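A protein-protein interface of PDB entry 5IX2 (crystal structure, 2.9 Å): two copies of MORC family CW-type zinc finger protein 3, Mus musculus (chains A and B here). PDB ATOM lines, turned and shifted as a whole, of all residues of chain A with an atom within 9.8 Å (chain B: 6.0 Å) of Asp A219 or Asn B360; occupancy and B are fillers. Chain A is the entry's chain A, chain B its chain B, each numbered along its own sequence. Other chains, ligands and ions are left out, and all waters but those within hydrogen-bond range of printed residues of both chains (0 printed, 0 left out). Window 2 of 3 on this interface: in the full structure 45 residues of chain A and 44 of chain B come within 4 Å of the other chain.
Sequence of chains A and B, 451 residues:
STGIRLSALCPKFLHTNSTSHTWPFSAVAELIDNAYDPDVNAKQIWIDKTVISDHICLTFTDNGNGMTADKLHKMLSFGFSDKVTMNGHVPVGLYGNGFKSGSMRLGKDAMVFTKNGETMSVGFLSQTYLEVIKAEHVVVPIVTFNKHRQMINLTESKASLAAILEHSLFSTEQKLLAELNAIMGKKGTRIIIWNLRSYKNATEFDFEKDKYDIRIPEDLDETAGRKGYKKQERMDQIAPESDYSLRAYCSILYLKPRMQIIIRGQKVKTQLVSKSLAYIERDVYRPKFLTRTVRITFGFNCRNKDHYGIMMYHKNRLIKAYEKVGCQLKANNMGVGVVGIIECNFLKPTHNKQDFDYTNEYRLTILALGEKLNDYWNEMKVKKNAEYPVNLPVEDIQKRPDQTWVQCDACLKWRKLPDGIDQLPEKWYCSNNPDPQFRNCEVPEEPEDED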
ATOM      1  N   THR A  22     -11.258  -1.608 -10.439  1.00  0.00           N
ATOM      2  CA  THR A  22     -11.258  -0.169 -10.495  1.00  0.00           C
ATOM      3  C   THR A  22     -10.139   0.413  -9.696  1.00  0.00           C
ATOM      4  O   THR A  22      -9.829   1.572  -9.799  1.00  0.00           O
ATOM      5  CB  THR A  22     -12.602   0.404 -10.057  1.00  0.00           C
ATOM      6  OG1 THR A  22     -12.895  -0.009  -8.729  1.00  0.00           O
ATOM      7  CG2 THR A  22     -13.657  -0.109 -10.934  1.00  0.00           C
ATOM      8  N   ARG A 105      -6.217  -5.818 -16.951  1.00  0.00           N
ATOM      9  CA  ARG A 105      -6.447  -4.596 -16.252  1.00  0.00           C
ATOM     10  C   ARG A 105      -5.145  -3.877 -16.223  1.00  0.00           C
ATOM     11  O   ARG A 105      -5.066  -2.697 -16.455  1.00  0.00           O
ATOM     12  CB  ARG A 105      -6.873  -4.894 -14.836  1.00  0.00           C
ATOM     13  CG  ARG A 105      -6.910  -3.694 -13.921  1.00  0.00           C
ATOM     14  CD  ARG A 105      -7.461  -2.488 -14.617  1.00  0.00           C
ATOM     15  NE  ARG A 105      -7.570  -1.379 -13.708  1.00  0.00           N
ATOM     16  CZ  ARG A 105      -6.747  -0.358 -13.701  1.00  0.00           C
ATOM     17  NH1 ARG A 105      -6.911   0.610 -12.841  1.00  0.00           N
ATOM     18  NH2 ARG A 105      -5.745  -0.319 -14.543  1.00  0.00           N
ATOM     19  N   SER A 198      -1.770   3.909 -19.457  1.00  0.00           N
ATOM     20  CA  SER A 198      -1.211   5.215 -19.260  1.00  0.00           C
ATOM     21  C   SER A 198      -2.275   6.256 -19.390  1.00  0.00           C
ATOM     22  O   SER A 198      -3.079   6.201 -20.294  1.00  0.00           O
ATOM     23  CB  SER A 198      -0.137   5.474 -20.298  1.00  0.00           C
ATOM     24  OG  SER A 198      -0.701   5.819 -21.544  1.00  0.00           O
ATOM     25  N   TYR A 199      -2.259   7.231 -18.501  1.00  0.00           N
ATOM     26  CA  TYR A 199      -3.097   8.392 -18.666  1.00  0.00           C
ATOM     27  C   TYR A 199      -2.192   9.567 -18.806  1.00  0.00           C
ATOM     28  O   TYR A 199      -1.227   9.713 -18.075  1.00  0.00           O
ATOM     29  CB  TYR A 199      -4.044   8.626 -17.504  1.00  0.00           C
ATOM     30  CG  TYR A 199      -4.917   9.838 -17.730  1.00  0.00           C
ATOM     31  CD1 TYR A 199      -5.591  10.012 -18.923  1.00  0.00           C
ATOM     32  CD2 TYR A 199      -5.045  10.815 -16.762  1.00  0.00           C
ATOM     33  CE1 TYR A 199      -6.381  11.116 -19.137  1.00  0.00           C
ATOM     34  CE2 TYR A 199      -5.833  11.926 -16.967  1.00  0.00           C
ATOM     35  CZ  TYR A 199      -6.499  12.072 -18.157  1.00  0.00           C
ATOM     36  OH  TYR A 199      -7.287  13.180 -18.365  1.00  0.00           O
ATOM     37  N   LYS A 200      -2.514  10.414 -19.763  1.00  0.00           N
ATOM     38  CA  LYS A 200      -1.600  11.426 -20.204  1.00  0.00           C
ATOM     39  C   LYS A 200      -0.467  10.636 -20.803  1.00  0.00           C
ATOM     40  O   LYS A 200      -0.738   9.685 -21.517  1.00  0.00           O
ATOM     41  CB  LYS A 200      -1.149  12.247 -19.010  1.00  0.00           C
ATOM     42  CG  LYS A 200      -2.265  12.475 -17.999  1.00  0.00           C
ATOM     43  CD  LYS A 200      -2.150  13.808 -17.293  1.00  0.00           C
ATOM     44  CE  LYS A 200      -3.277  14.741 -17.680  1.00  0.00           C
ATOM     45  NZ  LYS A 200      -3.047  16.106 -17.139  1.00  0.00           N
ATOM     46  N   GLU A 204       0.234   4.492 -15.398  1.00  0.00           N
ATOM     47  CA  GLU A 204      -0.718   4.743 -14.355  1.00  0.00           C
ATOM     48  C   GLU A 204      -0.061   4.735 -13.005  1.00  0.00           C
ATOM     49  O   GLU A 204      -0.430   5.490 -12.151  1.00  0.00           O
ATOM     50  CB  GLU A 204      -1.760   3.643 -14.415  1.00  0.00           C
ATOM     51  CG  GLU A 204      -2.616   3.484 -13.186  1.00  0.00           C
ATOM     52  CD  GLU A 204      -3.656   2.428 -13.372  1.00  0.00           C
ATOM     53  OE1 GLU A 204      -3.339   1.379 -13.924  1.00  0.00           O
ATOM     54  OE2 GLU A 204      -4.797   2.652 -12.981  1.00  0.00           O
ATOM     55  N   ASP A 206       3.110   5.202 -10.299  1.00  0.00           N
ATOM     56  CA  ASP A 206       4.216   6.101 -10.090  1.00  0.00           C
ATOM     57  C   ASP A 206       5.369   5.318  -9.537  1.00  0.00           C
ATOM     58  O   ASP A 206       5.283   4.779  -8.455  1.00  0.00           O
ATOM     59  CB  ASP A 206       3.827   7.126  -9.054  1.00  0.00           C
ATOM     60  CG  ASP A 206       4.831   8.207  -8.904  1.00  0.00           C
ATOM     61  OD1 ASP A 206       5.708   8.327  -9.754  1.00  0.00           O
ATOM     62  OD2 ASP A 206       4.739   8.963  -7.939  1.00  0.00           O
ATOM     63  N   LYS A 209       8.428   8.123  -7.203  1.00  0.00           N
ATOM     64  CA  LYS A 209       8.314   8.608  -5.850  1.00  0.00           C
ATOM     65  C   LYS A 209       9.056   7.769  -4.854  1.00  0.00           C
ATOM     66  O   LYS A 209       9.606   8.276  -3.910  1.00  0.00           O
ATOM     67  CB  LYS A 209       6.861   8.661  -5.445  1.00  0.00           C
ATOM     68  CG  LYS A 209       6.606   9.522  -4.239  1.00  0.00           C
ATOM     69  CD  LYS A 209       5.965  10.808  -4.682  1.00  0.00           C
ATOM     70  CE  LYS A 209       6.088  11.881  -3.630  1.00  0.00           C
ATOM     71  NZ  LYS A 209       5.895  11.294  -2.288  1.00  0.00           N
ATOM     72  N   ILE A 216       0.346   4.682  -6.469  1.00  0.00           N
ATOM     73  CA  ILE A 216      -0.633   5.394  -7.255  1.00  0.00           C
ATOM     74  C   ILE A 216      -0.435   6.849  -6.989  1.00  0.00           C
ATOM     75  O   ILE A 216      -0.321   7.264  -5.855  1.00  0.00           O
ATOM     76  CB  ILE A 216      -2.074   5.066  -6.878  1.00  0.00           C
ATOM     77  CG1 ILE A 216      -2.364   3.592  -7.021  1.00  0.00           C
ATOM     78  CG2 ILE A 216      -3.007   5.766  -7.820  1.00  0.00           C
ATOM     79  CD1 ILE A 216      -3.507   3.134  -6.168  1.00  0.00           C
ATOM     80  N   PRO A 217      -0.383   7.641  -8.139  1.00  0.00           N
ATOM     81  CA  PRO A 217      -0.030   9.031  -7.870  1.00  0.00           C
ATOM     82  C   PRO A 217      -1.101   9.839  -7.182  1.00  0.00           C
ATOM     83  O   PRO A 217      -2.257   9.694  -7.472  1.00  0.00           O
ATOM     84  CB  PRO A 217       0.187   9.618  -9.256  1.00  0.00           C
ATOM     85  CG  PRO A 217       0.389   8.494 -10.159  1.00  0.00           C
ATOM     86  CD  PRO A 217      -0.613   7.558  -9.659  1.00  0.00           C
ATOM     87  N   GLU A 218      -0.698  10.735  -6.305  1.00  0.00           N
ATOM     88  CA  GLU A 218      -1.597  11.748  -5.815  1.00  0.00           C
ATOM     89  C   GLU A 218      -1.822  12.672  -6.971  1.00  0.00           C
ATOM     90  O   GLU A 218      -0.973  12.787  -7.825  1.00  0.00           O
ATOM     91  CB  GLU A 218      -0.966  12.531  -4.671  1.00  0.00           C
ATOM     92  CG  GLU A 218       0.550  12.475  -4.613  1.00  0.00           C
ATOM     93  CD  GLU A 218       1.111  13.215  -3.414  1.00  0.00           C
ATOM     94  OE1 GLU A 218       0.788  14.407  -3.256  1.00  0.00           O
ATOM     95  OE2 GLU A 218       1.871  12.610  -2.627  1.00  0.00           O
ATOM     96  N   ASP A 219      -2.966  13.326  -7.021  1.00  0.00           N
ATOM     97  CA  ASP A 219      -3.174  14.340  -8.038  1.00  0.00           C
ATOM     98  C   ASP A 219      -4.030  15.492  -7.534  1.00  0.00           C
ATOM     99  O   ASP A 219      -3.707  16.657  -7.760  1.00  0.00           O
ATOM    100  CB  ASP A 219      -3.766  13.748  -9.303  1.00  0.00           C
ATOM    101  CG  ASP A 219      -3.731  14.719 -10.451  1.00  0.00           C
ATOM    102  OD1 ASP A 219      -3.882  15.928 -10.199  1.00  0.00           O
ATOM    103  OD2 ASP A 219      -3.537  14.285 -11.605  1.00  0.00           O
ATOM    104  N   TYR A 229      -4.199  10.003  -2.725  1.00  0.00           N
ATOM    105  CA  TYR A 229      -5.151   9.162  -3.423  1.00  0.00           C
ATOM    106  C   TYR A 229      -5.939   8.297  -2.463  1.00  0.00           C
ATOM    107  O   TYR A 229      -5.373   7.610  -1.645  1.00  0.00           O
ATOM    108  CB  TYR A 229      -4.439   8.285  -4.446  1.00  0.00           C
ATOM    109  CG  TYR A 229      -5.302   7.193  -5.007  1.00  0.00           C
ATOM    110  CD1 TYR A 229      -5.615   6.099  -4.257  1.00  0.00           C
ATOM    111  CD2 TYR A 229      -5.831   7.285  -6.258  1.00  0.00           C
ATOM    112  CE1 TYR A 229      -6.413   5.108  -4.755  1.00  0.00           C
ATOM    113  CE2 TYR A 229      -6.630   6.299  -6.757  1.00  0.00           C
ATOM    114  CZ  TYR A 229      -6.914   5.220  -6.000  1.00  0.00           C
ATOM    115  OH  TYR A 229      -7.707   4.261  -6.530  1.00  0.00           O
ATOM    116  N   LYS A 230      -7.255   8.297  -2.619  1.00  0.00           N
ATOM    117  CA  LYS A 230      -8.103   7.465  -1.798  1.00  0.00           C
ATOM    118  C   LYS A 230      -8.998   6.669  -2.691  1.00  0.00           C
ATOM    119  O   LYS A 230      -9.329   7.095  -3.765  1.00  0.00           O
ATOM    120  CB  LYS A 230      -8.938   8.294  -0.829  1.00  0.00           C
ATOM    121  CG  LYS A 230      -8.974   9.782  -1.113  1.00  0.00           C
ATOM    122  CD  LYS A 230      -9.356  10.577   0.121  1.00  0.00           C
ATOM    123  CE  LYS A 230      -9.061  12.054  -0.062  1.00  0.00           C
ATOM    124  NZ  LYS A 230      -7.885  12.501   0.735  1.00  0.00           N
ATOM    125  N   TYR A 244      -2.791   3.510  -1.530  1.00  0.00           N
ATOM    126  CA  TYR A 244      -1.875   4.056  -2.505  1.00  0.00           C
ATOM    127  C   TYR A 244      -0.480   3.474  -2.559  1.00  0.00           C
ATOM    128  O   TYR A 244       0.250   3.779  -3.461  1.00  0.00           O
ATOM    129  CB  TYR A 244      -1.808   5.563  -2.356  1.00  0.00           C
ATOM    130  CG  TYR A 244      -1.319   6.027  -1.024  1.00  0.00           C
ATOM    131  CD1 TYR A 244      -0.082   6.597  -0.893  1.00  0.00           C
ATOM    132  CD2 TYR A 244      -2.097   5.919   0.093  1.00  0.00           C
ATOM    133  CE1 TYR A 244       0.376   7.028   0.323  1.00  0.00           C
ATOM    134  CE2 TYR A 244      -1.642   6.346   1.315  1.00  0.00           C
ATOM    135  CZ  TYR A 244      -0.403   6.904   1.415  1.00  0.00           C
ATOM    136  OH  TYR A 244       0.074   7.337   2.615  1.00  0.00           O
ATOM    137  N   TYR B 358     -12.804   4.381 -11.921  1.00  0.00           N
ATOM    138  CA  TYR B 358     -12.445   5.431 -11.003  1.00  0.00           C
ATOM    139  C   TYR B 358     -11.193   6.157 -11.436  1.00  0.00           C
ATOM    140  O   TYR B 358     -10.185   6.146 -10.772  1.00  0.00           O
ATOM    141  CB  TYR B 358     -12.246   4.815  -9.636  1.00  0.00           C
ATOM    142  CG  TYR B 358     -12.183   5.784  -8.511  1.00  0.00           C
ATOM    143  CD1 TYR B 358     -12.921   6.923  -8.516  1.00  0.00           C
ATOM    144  CD2 TYR B 358     -11.396   5.540  -7.433  1.00  0.00           C
ATOM    145  CE1 TYR B 358     -12.857   7.806  -7.477  1.00  0.00           C
ATOM    146  CE2 TYR B 358     -11.326   6.419  -6.392  1.00  0.00           C
ATOM    147  CZ  TYR B 358     -12.057   7.552  -6.429  1.00  0.00           C
ATOM    148  OH  TYR B 358     -11.987   8.420  -5.390  1.00  0.00           O
ATOM    149  N   THR B 359     -11.301   6.819 -12.563  1.00  0.00           N
ATOM    150  CA  THR B 359     -10.226   7.540 -13.164  1.00  0.00           C
ATOM    151  C   THR B 359     -10.099   8.909 -12.604  1.00  0.00           C
ATOM    152  O   THR B 359     -10.867   9.301 -11.781  1.00  0.00           O
ATOM    153  CB  THR B 359     -10.429   7.650 -14.652  1.00  0.00           C
ATOM    154  OG1 THR B 359     -11.612   8.385 -14.904  1.00  0.00           O
ATOM    155  CG2 THR B 359     -10.571   6.305 -15.217  1.00  0.00           C
ATOM    156  N   ASN B 360      -9.079   9.623 -13.029  1.00  0.00           N
ATOM    157  CA  ASN B 360      -8.878  10.986 -12.621  1.00  0.00           C
ATOM    158  C   ASN B 360     -10.011  11.830 -13.093  1.00  0.00           C
ATOM    159  O   ASN B 360     -10.461  12.716 -12.405  1.00  0.00           O
ATOM    160  CB  ASN B 360      -7.600  11.511 -13.244  1.00  0.00           C
ATOM    161  CG  ASN B 360      -7.289  12.924 -12.833  1.00  0.00           C
ATOM    162  OD1 ASN B 360      -7.193  13.232 -11.659  1.00  0.00           O
ATOM    163  ND2 ASN B 360      -7.116  13.785 -13.804  1.00  0.00           N
ATOM    164  N   GLU B 361     -10.449  11.557 -14.302  1.00  0.00           N
ATOM    165  CA  GLU B 361     -11.540  12.280 -14.896  1.00  0.00           C
ATOM    166  C   GLU B 361     -12.838  12.096 -14.141  1.00  0.00           C
ATOM    167  O   GLU B 361     -13.616  13.014 -14.041  1.00  0.00           O
ATOM    168  CB  GLU B 361     -11.678  11.905 -16.357  1.00  0.00           C
ATOM    169  CG  GLU B 361     -10.372  12.004 -17.110  1.00  0.00           C
ATOM    170  CD  GLU B 361     -10.549  12.079 -18.604  1.00  0.00           C
ATOM    171  OE1 GLU B 361      -9.740  12.738 -19.268  1.00  0.00           O
ATOM    172  OE2 GLU B 361     -11.488  11.472 -19.123  1.00  0.00           O
ATOM    173  N   TYR B 362     -13.101  10.904 -13.660  1.00  0.00           N
ATOM    174  CA  TYR B 362     -14.270  10.711 -12.850  1.00  0.00           C
ATOM    175  C   TYR B 362     -14.172  11.477 -11.571  1.00  0.00           C
ATOM    176  O   TYR B 362     -15.119  12.065 -11.132  1.00  0.00           O
ATOM    177  CB  TYR B 362     -14.489   9.243 -12.556  1.00  0.00           C
ATOM    178  CG  TYR B 362     -15.556   8.980 -11.536  1.00  0.00           C
ATOM    179  CD1 TYR B 362     -16.806   8.570 -11.915  1.00  0.00           C
ATOM    180  CD2 TYR B 362     -15.308   9.140 -10.195  1.00  0.00           C
ATOM    181  CE1 TYR B 362     -17.780   8.320 -10.990  1.00  0.00           C
ATOM    182  CE2 TYR B 362     -16.283   8.899  -9.265  1.00  0.00           C
ATOM    183  CZ  TYR B 362     -17.513   8.488  -9.679  1.00  0.00           C
ATOM    184  OH  TYR B 362     -18.481   8.240  -8.763  1.00  0.00           O
ATOM    185  N   ARG B 363     -13.010  11.464 -10.964  1.00  0.00           N
ATOM    186  CA  ARG B 363     -12.823  12.144  -9.710  1.00  0.00           C
ATOM    187  C   ARG B 363     -13.025  13.609  -9.908  1.00  0.00           C
ATOM    188  O   ARG B 363     -13.588  14.286  -9.090  1.00  0.00           O
ATOM    189  CB  ARG B 363     -11.425  11.896  -9.207  1.00  0.00           C
ATOM    190  CG  ARG B 363     -11.301  10.643  -8.384  1.00  0.00           C
ATOM    191  CD  ARG B 363      -9.957  10.573  -7.701  1.00  0.00           C
ATOM    192  NE  ARG B 363      -8.882  10.472  -8.663  1.00  0.00           N
ATOM    193  CZ  ARG B 363      -8.497   9.337  -9.202  1.00  0.00           C
ATOM    194  NH1 ARG B 363      -9.095   8.226  -8.860  1.00  0.00           N
ATOM    195  NH2 ARG B 363      -7.513   9.315 -10.070  1.00  0.00           N
ATOM    196  N   LEU B 364     -12.517  14.102 -11.006  1.00  0.00           N
ATOM    197  CA  LEU B 364     -12.652  15.489 -11.321  1.00  0.00           C
ATOM    198  C   LEU B 364     -14.097  15.843 -11.529  1.00  0.00           C
ATOM    199  O   LEU B 364     -14.549  16.882 -11.111  1.00  0.00           O
ATOM    200  CB  LEU B 364     -11.859  15.790 -12.569  1.00  0.00           C
ATOM    201  CG  LEU B 364     -10.398  16.112 -12.357  1.00  0.00           C
ATOM    202  CD1 LEU B 364      -9.908  16.774 -13.612  1.00  0.00           C
ATOM    203  CD2 LEU B 364     -10.221  17.044 -11.183  1.00  0.00           C
ATOM    204  N   THR B 365     -14.829  14.976 -12.197  1.00  0.00           N
ATOM    205  CA  THR B 365     -16.220  15.232 -12.451  1.00  0.00           C
ATOM    206  C   THR B 365     -16.989  15.291 -11.167  1.00  0.00           C
ATOM    207  O   THR B 365     -17.817  16.139 -10.978  1.00  0.00           O
ATOM    208  CB  THR B 365     -16.813  14.139 -13.313  1.00  0.00           C
ATOM    209  OG1 THR B 365     -16.124  14.118 -14.549  1.00  0.00           O
ATOM    210  CG2 THR B 365     -18.207  14.437 -13.603  1.00  0.00           C
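OH of Tyr A199 sits at hydrogen-bond distance from OE1 of Glu B361.
The side-chain hydroxyl of Tyr B358 lies close to the backbone carbonyl oxygen of Lys A230.
The side-chain hydroxyl (OG1) of Thr B365 lies within hydrogen-bond range of the backbone carbonyl oxygen (O) of Glu B361, 2.8 Å away.
The side-chain hydroxyl (OG1) of Thr B359 sits close to the backbone NH (N) of Glu B361 (3.4 Å).
NH1 of Arg B363 sits at hydrogen-bond distance from O of Tyr B358 (3.0 Å).
Among the printed residues, pairs that only touch across the chains: Tyr A229 with Arg B363 (3.8 Å), Asp A219 with Asn B360 (3.8 Å) and Tyr A199 with Asn B360 (3.9 Å).
Of chain B, only Asn B360 comes within 4 Å of Asp A219.
Of chain A, only Tyr A199 and Asp A219 come within 4 Å of Asn B360.
Of the printed residues of chain B, Tyr A229 touches Arg B363 (3.8 Å).
Printed residues of chain B within 4 Å of Lys A230: Tyr B358 (3.4 Å).
Of the printed residues of chain A, Glu B361 touches Tyr A199 (2.7 Å).
Thr B365 touches none of the printed residues of chain A.
Ile A216 touches none of the printed residues of chain B.
The nearest residue of chain B that does not touch Asp A219 is Arg B363 (5.9 Å).
Of the 8 printed residues of chain B, 4 touch a printed residue of chain A.
Among the printed residues, 5 pairs touch across the chains.
Among the printed residues, no Asp or Glu carboxylate lies within 4 Å of a Lys or Arg side-chain nitrogen of the other chain.
No position is printed for both chains.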
